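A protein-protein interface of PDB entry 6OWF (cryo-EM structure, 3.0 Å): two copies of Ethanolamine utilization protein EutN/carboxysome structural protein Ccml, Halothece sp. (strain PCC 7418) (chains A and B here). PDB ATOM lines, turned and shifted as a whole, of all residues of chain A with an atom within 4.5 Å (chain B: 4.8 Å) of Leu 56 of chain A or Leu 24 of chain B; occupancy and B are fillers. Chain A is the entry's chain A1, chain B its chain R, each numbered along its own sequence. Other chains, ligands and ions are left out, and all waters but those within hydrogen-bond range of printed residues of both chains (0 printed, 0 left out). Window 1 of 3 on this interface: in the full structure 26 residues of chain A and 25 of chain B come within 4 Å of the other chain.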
ATOM      1  N   MET A   1     -26.579  -1.446 -19.896  1.00  0.00           N
ATOM      2  CA  MET A   1     -25.584  -0.416 -19.631  1.00  0.00           C
ATOM      3  C   MET A   1     -24.189  -0.887 -20.006  1.00  0.00           C
ATOM      4  O   MET A   1     -23.902  -2.078 -20.007  1.00  0.00           O
ATOM      5  CB  MET A   1     -25.617  -0.007 -18.160  1.00  0.00           C
ATOM      6  CG  MET A   1     -26.728   0.956 -17.792  1.00  0.00           C
ATOM      7  SD  MET A   1     -28.361   0.202 -17.853  1.00  0.00           S
ATOM      8  CE  MET A   1     -28.272  -0.931 -16.478  1.00  0.00           C
ATOM      9  N   GLN A   2     -23.329   0.068 -20.335  1.00  0.00           N
ATOM     10  CA  GLN A   2     -21.930  -0.189 -20.626  1.00  0.00           C
ATOM     11  C   GLN A   2     -21.081   0.784 -19.828  1.00  0.00           C
ATOM     12  O   GLN A   2     -21.446   1.947 -19.659  1.00  0.00           O
ATOM     13  CB  GLN A   2     -21.622  -0.026 -22.114  1.00  0.00           C
ATOM     14  CG  GLN A   2     -22.187  -1.103 -23.009  1.00  0.00           C
ATOM     15  CD  GLN A   2     -21.343  -2.352 -23.012  1.00  0.00           C
ATOM     16  OE1 GLN A   2     -21.790  -3.415 -22.593  1.00  0.00           O
ATOM     17  NE2 GLN A   2     -20.111  -2.232 -23.486  1.00  0.00           N
ATOM     18  N   MET A   3     -19.946   0.305 -19.335  1.00  0.00           N
ATOM     19  CA  MET A   3     -18.982   1.180 -18.688  1.00  0.00           C
ATOM     20  C   MET A   3     -18.183   1.891 -19.767  1.00  0.00           C
ATOM     21  O   MET A   3     -17.728   1.262 -20.725  1.00  0.00           O
ATOM     22  CB  MET A   3     -18.050   0.397 -17.765  1.00  0.00           C
ATOM     23  CG  MET A   3     -18.752  -0.556 -16.825  1.00  0.00           C
ATOM     24  SD  MET A   3     -17.649  -1.158 -15.537  1.00  0.00           S
ATOM     25  CE  MET A   3     -16.325  -1.836 -16.525  1.00  0.00           C
ATOM     26  N   VAL A  55     -18.147   6.297 -16.598  1.00  0.00           N
ATOM     27  CA  VAL A  55     -19.591   6.456 -16.524  1.00  0.00           C
ATOM     28  C   VAL A  55     -20.275   5.178 -16.987  1.00  0.00           C
ATOM     29  O   VAL A  55     -19.661   4.293 -17.583  1.00  0.00           O
ATOM     30  CB  VAL A  55     -20.090   7.654 -17.358  1.00  0.00           C
ATOM     31  CG1 VAL A  55     -19.633   8.958 -16.747  1.00  0.00           C
ATOM     32  CG2 VAL A  55     -19.614   7.543 -18.786  1.00  0.00           C
ATOM     33  N   LEU A  56     -21.567   5.092 -16.688  1.00  0.00           N
ATOM     34  CA  LEU A  56     -22.431   4.026 -17.178  1.00  0.00           C
ATOM     35  C   LEU A  56     -23.341   4.602 -18.252  1.00  0.00           C
ATOM     36  O   LEU A  56     -24.131   5.508 -17.977  1.00  0.00           O
ATOM     37  CB  LEU A  56     -23.266   3.430 -16.049  1.00  0.00           C
ATOM     38  CG  LEU A  56     -22.747   2.182 -15.348  1.00  0.00           C
ATOM     39  CD1 LEU A  56     -23.775   1.705 -14.354  1.00  0.00           C
ATOM     40  CD2 LEU A  56     -22.444   1.101 -16.354  1.00  0.00           C
ATOM     41  N   VAL A  57     -23.234   4.080 -19.468  1.00  0.00           N
ATOM     42  CA  VAL A  57     -23.995   4.583 -20.601  1.00  0.00           C
ATOM     43  C   VAL A  57     -24.913   3.483 -21.121  1.00  0.00           C
ATOM     44  O   VAL A  57     -24.502   2.327 -21.266  1.00  0.00           O
ATOM     45  CB  VAL A  57     -23.054   5.146 -21.695  1.00  0.00           C
ATOM     46  CG1 VAL A  57     -22.009   4.140 -22.134  1.00  0.00           C
ATOM     47  CG2 VAL A  57     -23.835   5.647 -22.894  1.00  0.00           C
ATOM     48  N   ASN A  58     -26.179   3.831 -21.336  1.00  0.00           N
ATOM     49  CA  ASN A  58     -27.166   2.904 -21.864  1.00  0.00           C
ATOM     50  C   ASN A  58     -27.562   3.327 -23.269  1.00  0.00           C
ATOM     51  O   ASN A  58     -27.600   4.516 -23.586  1.00  0.00           O
ATOM     52  CB  ASN A  58     -28.404   2.827 -20.966  1.00  0.00           C
ATOM     53  CG  ASN A  58     -29.086   4.160 -20.788  1.00  0.00           C
ATOM     54  OD1 ASN A  58     -28.479   5.207 -20.953  1.00  0.00           O
ATOM     55  ND2 ASN A  58     -30.355   4.126 -20.426  1.00  0.00           N
ATOM     56  N   MET A  77     -27.244   7.764 -23.377  1.00  0.00           N
ATOM     57  CA  MET A  77     -27.339   8.681 -22.253  1.00  0.00           C
ATOM     58  C   MET A  77     -26.448   8.159 -21.137  1.00  0.00           C
ATOM     59  O   MET A  77     -26.241   6.956 -21.014  1.00  0.00           O
ATOM     60  CB  MET A  77     -28.799   8.812 -21.799  1.00  0.00           C
ATOM     61  CG  MET A  77     -29.082   9.865 -20.764  1.00  0.00           C
ATOM     62  SD  MET A  77     -30.831  10.058 -20.405  1.00  0.00           S
ATOM     63  CE  MET A  77     -31.162   8.523 -19.560  1.00  0.00           C
ATOM     64  N   VAL A  78     -25.911   9.068 -20.333  1.00  0.00           N
ATOM     65  CA  VAL A  78     -25.106   8.709 -19.173  1.00  0.00           C
ATOM     66  C   VAL A  78     -26.060   8.644 -17.988  1.00  0.00           C
ATOM     67  O   VAL A  78     -26.651   9.651 -17.594  1.00  0.00           O
ATOM     68  CB  VAL A  78     -23.972   9.708 -18.939  1.00  0.00           C
ATOM     69  CG1 VAL A  78     -23.339   9.473 -17.590  1.00  0.00           C
ATOM     70  CG2 VAL A  78     -22.940   9.593 -20.035  1.00  0.00           C
ATOM     71  N   VAL A  79     -26.230   7.448 -17.424  1.00  0.00           N
ATOM     72  CA  VAL A  79     -27.206   7.284 -16.354  1.00  0.00           C
ATOM     73  C   VAL A  79     -26.530   7.315 -14.991  1.00  0.00           C
ATOM     74  O   VAL A  79     -27.174   7.593 -13.975  1.00  0.00           O
ATOM     75  CB  VAL A  79     -28.017   5.993 -16.553  1.00  0.00           C
ATOM     76  CG1 VAL A  79     -28.874   6.109 -17.780  1.00  0.00           C
ATOM     77  CG2 VAL A  79     -27.103   4.793 -16.658  1.00  0.00           C
ATOM     78  N   ALA A  80     -25.231   7.043 -14.941  1.00  0.00           N
ATOM     79  CA  ALA A  80     -24.547   6.962 -13.662  1.00  0.00           C
ATOM     80  C   ALA A  80     -23.075   7.276 -13.845  1.00  0.00           C
ATOM     81  O   ALA A  80     -22.464   6.928 -14.856  1.00  0.00           O
ATOM     82  CB  ALA A  80     -24.706   5.577 -13.024  1.00  0.00           C
ATOM     83  N   ILE A  82     -19.703   6.122 -12.308  1.00  0.00           N
ATOM     84  CA  ILE A  82     -19.316   4.903 -11.616  1.00  0.00           C
ATOM     85  C   ILE A  82     -18.448   5.254 -10.416  1.00  0.00           C
ATOM     86  O   ILE A  82     -17.422   5.935 -10.543  1.00  0.00           O
ATOM     87  CB  ILE A  82     -18.601   3.951 -12.585  1.00  0.00           C
ATOM     88  CG1 ILE A  82     -19.627   3.213 -13.437  1.00  0.00           C
ATOM     89  CG2 ILE A  82     -17.761   2.945 -11.845  1.00  0.00           C
ATOM     90  CD1 ILE A  82     -19.015   2.410 -14.549  1.00  0.00           C
ATOM     91  N   THR B   9     -19.691  -6.544  -9.694  1.00  0.00           N
ATOM     92  CA  THR B   9     -20.683  -5.571  -9.268  1.00  0.00           C
ATOM     93  C   THR B   9     -20.208  -4.171  -9.640  1.00  0.00           C
ATOM     94  O   THR B   9     -19.023  -3.857  -9.510  1.00  0.00           O
ATOM     95  CB  THR B   9     -20.901  -5.697  -7.754  1.00  0.00           C
ATOM     96  OG1 THR B   9     -21.334  -7.027  -7.451  1.00  0.00           O
ATOM     97  CG2 THR B   9     -21.950  -4.749  -7.264  1.00  0.00           C
ATOM     98  N   VAL B  10     -21.130  -3.331 -10.106  1.00  0.00           N
ATOM     99  CA  VAL B  10     -20.859  -1.929 -10.400  1.00  0.00           C
ATOM    100  C   VAL B  10     -21.754  -1.081  -9.508  1.00  0.00           C
ATOM    101  O   VAL B  10     -22.972  -1.280  -9.475  1.00  0.00           O
ATOM    102  CB  VAL B  10     -21.094  -1.611 -11.887  1.00  0.00           C
ATOM    103  CG1 VAL B  10     -20.968  -0.124 -12.147  1.00  0.00           C
ATOM    104  CG2 VAL B  10     -20.114  -2.380 -12.748  1.00  0.00           C
ATOM    105  N   GLY B  12     -22.670   2.929  -8.477  1.00  0.00           N
ATOM    106  CA  GLY B  12     -22.546   4.342  -8.765  1.00  0.00           C
ATOM    107  C   GLY B  12     -23.422   5.169  -7.851  1.00  0.00           C
ATOM    108  O   GLY B  12     -24.622   4.910  -7.743  1.00  0.00           O
ATOM    109  N   MET B  19     -32.595   5.884 -11.193  1.00  0.00           N
ATOM    110  CA  MET B  19     -31.703   4.742 -11.072  1.00  0.00           C
ATOM    111  C   MET B  19     -31.435   4.343  -9.630  1.00  0.00           C
ATOM    112  O   MET B  19     -30.563   3.501  -9.395  1.00  0.00           O
ATOM    113  CB  MET B  19     -30.379   5.049 -11.768  1.00  0.00           C
ATOM    114  CG  MET B  19     -30.476   5.084 -13.275  1.00  0.00           C
ATOM    115  SD  MET B  19     -30.603   3.438 -13.978  1.00  0.00           S
ATOM    116  CE  MET B  19     -28.974   2.805 -13.603  1.00  0.00           C
ATOM    117  N   VAL B  22     -31.612   0.339  -7.887  1.00  0.00           N
ATOM    118  CA  VAL B  22     -31.399  -0.618  -8.962  1.00  0.00           C
ATOM    119  C   VAL B  22     -30.036  -1.259  -8.755  1.00  0.00           C
ATOM    120  O   VAL B  22     -29.012  -0.569  -8.731  1.00  0.00           O
ATOM    121  CB  VAL B  22     -31.494   0.056 -10.338  1.00  0.00           C
ATOM    122  CG1 VAL B  22     -31.026  -0.887 -11.425  1.00  0.00           C
ATOM    123  CG2 VAL B  22     -32.914   0.494 -10.598  1.00  0.00           C
ATOM    124  N   LYS B  23     -30.028  -2.575  -8.590  1.00  0.00           N
ATOM    125  CA  LYS B  23     -28.796  -3.319  -8.379  1.00  0.00           C
ATOM    126  C   LYS B  23     -28.119  -3.553  -9.723  1.00  0.00           C
ATOM    127  O   LYS B  23     -28.676  -4.229 -10.592  1.00  0.00           O
ATOM    128  CB  LYS B  23     -29.108  -4.637  -7.678  1.00  0.00           C
ATOM    129  CG  LYS B  23     -27.987  -5.639  -7.651  1.00  0.00           C
ATOM    130  CD  LYS B  23     -28.490  -6.939  -7.061  1.00  0.00           C
ATOM    131  CE  LYS B  23     -27.386  -7.966  -6.946  1.00  0.00           C
ATOM    132  NZ  LYS B  23     -27.930  -9.274  -6.502  1.00  0.00           N
ATOM    133  N   LEU B  24     -26.928  -2.991  -9.898  1.00  0.00           N
ATOM    134  CA  LEU B  24     -26.208  -3.057 -11.161  1.00  0.00           C
ATOM    135  C   LEU B  24     -25.126  -4.118 -11.075  1.00  0.00           C
ATOM    136  O   LEU B  24     -24.173  -3.979 -10.304  1.00  0.00           O
ATOM    137  CB  LEU B  24     -25.584  -1.706 -11.507  1.00  0.00           C
ATOM    138  CG  LEU B  24     -26.537  -0.517 -11.593  1.00  0.00           C
ATOM    139  CD1 LEU B  24     -25.813   0.766 -11.247  1.00  0.00           C
ATOM    140  CD2 LEU B  24     -27.139  -0.435 -12.970  1.00  0.00           C
ATOM    141  N   LEU B  25     -25.268  -5.166 -11.874  1.00  0.00           N
ATOM    142  CA  LEU B  25     -24.309  -6.255 -11.926  1.00  0.00           C
ATOM    143  C   LEU B  25     -23.259  -5.979 -12.987  1.00  0.00           C
ATOM    144  O   LEU B  25     -23.301  -4.975 -13.694  1.00  0.00           O
ATOM    145  CB  LEU B  25     -25.007  -7.581 -12.221  1.00  0.00           C
ATOM    146  CG  LEU B  25     -25.858  -8.172 -11.110  1.00  0.00           C
ATOM    147  CD1 LEU B  25     -26.336  -9.531 -11.547  1.00  0.00           C
ATOM    148  CD2 LEU B  25     -25.049  -8.270  -9.837  1.00  0.00           C
ATOM    149  N   LEU B  26     -22.302  -6.888 -13.086  1.00  0.00           N
ATOM    150  CA  LEU B  26     -21.303  -6.863 -14.145  1.00  0.00           C
ATOM    151  C   LEU B  26     -21.222  -8.265 -14.718  1.00  0.00           C
ATOM    152  O   LEU B  26     -20.543  -9.132 -14.162  1.00  0.00           O
ATOM    153  CB  LEU B  26     -19.950  -6.393 -13.626  1.00  0.00           C
ATOM    154  CG  LEU B  26     -18.860  -6.300 -14.686  1.00  0.00           C
ATOM    155  CD1 LEU B  26     -19.276  -5.330 -15.743  1.00  0.00           C
ATOM    156  CD2 LEU B  26     -17.577  -5.851 -14.063  1.00  0.00           C
ATOM    157  N   VAL B  42     -23.427  -4.376 -18.155  1.00  0.00           N
ATOM    158  CA  VAL B  42     -23.887  -3.992 -16.827  1.00  0.00           C
ATOM    159  C   VAL B  42     -25.406  -4.021 -16.852  1.00  0.00           C
ATOM    160  O   VAL B  42     -26.036  -3.262 -17.597  1.00  0.00           O
ATOM    161  CB  VAL B  42     -23.362  -2.608 -16.419  1.00  0.00           C
ATOM    162  CG1 VAL B  42     -24.056  -2.127 -15.161  1.00  0.00           C
ATOM    163  CG2 VAL B  42     -21.867  -2.659 -16.216  1.00  0.00           C
ATOM    164  N   ALA B  43     -25.996  -4.903 -16.054  1.00  0.00           N
ATOM    165  CA  ALA B  43     -27.419  -5.183 -16.143  1.00  0.00           C
ATOM    166  C   ALA B  43     -28.089  -5.013 -14.791  1.00  0.00           C
ATOM    167  O   ALA B  43     -27.490  -5.269 -13.746  1.00  0.00           O
ATOM    168  CB  ALA B  43     -27.668  -6.598 -16.656  1.00  0.00           C
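The backbone carbonyl oxygen (O) of Val 42 of chain B sits at hydrogen-bond distance from the backbone NH (N) of Met 1 of chain A.
N of Val 10 of chain B lies within hydrogen-bond range of O of Leu 24 of chain B. N of Val 79 of chain A sits at hydrogen-bond distance from O of Leu 56 of chain A, 2.9 Å away. O of Ala 80 of chain A is in hydrogen-bond range of N of Leu 56 of chain A (2.7 Å).
Among the printed residues, merely in contact across the chains: Met 1 of chain A with Leu 24 of chain B (3.7 Å), Met 3 of chain A with Val 10 of chain B (3.9 Å), Met 3 of chain A with Val 42 of chain B (3.8 Å), Leu 56 of chain A with Leu 24 of chain B (3.8 Å), Leu 56 of chain A with Val 42 of chain B (3.8 Å) and Ile 82 of chain A with Val 10 of chain B (3.8 Å).
Printed residues of chain B within 4 Å of Ile 82 of chain A: Val 10. Printed residues of chain A within 4 Å of Val 10 of chain B: Met 3 (3.9 Å) and Ile 82 (3.8 Å).
Of the 11 printed residues of chain B, 3 touch a printed residue of chain A. Printed residues of chain B that touch a printed residue of chain A: Val 10, Leu 24 and Val 42. Along chain B the printed residues that touch a printed residue of chain A span positions 10 to 42. Among the printed residues, no Asp or Glu carboxylate lies within 4 Å of a Lys or Arg side-chain nitrogen of the other chain.
No position is printed for both chains.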
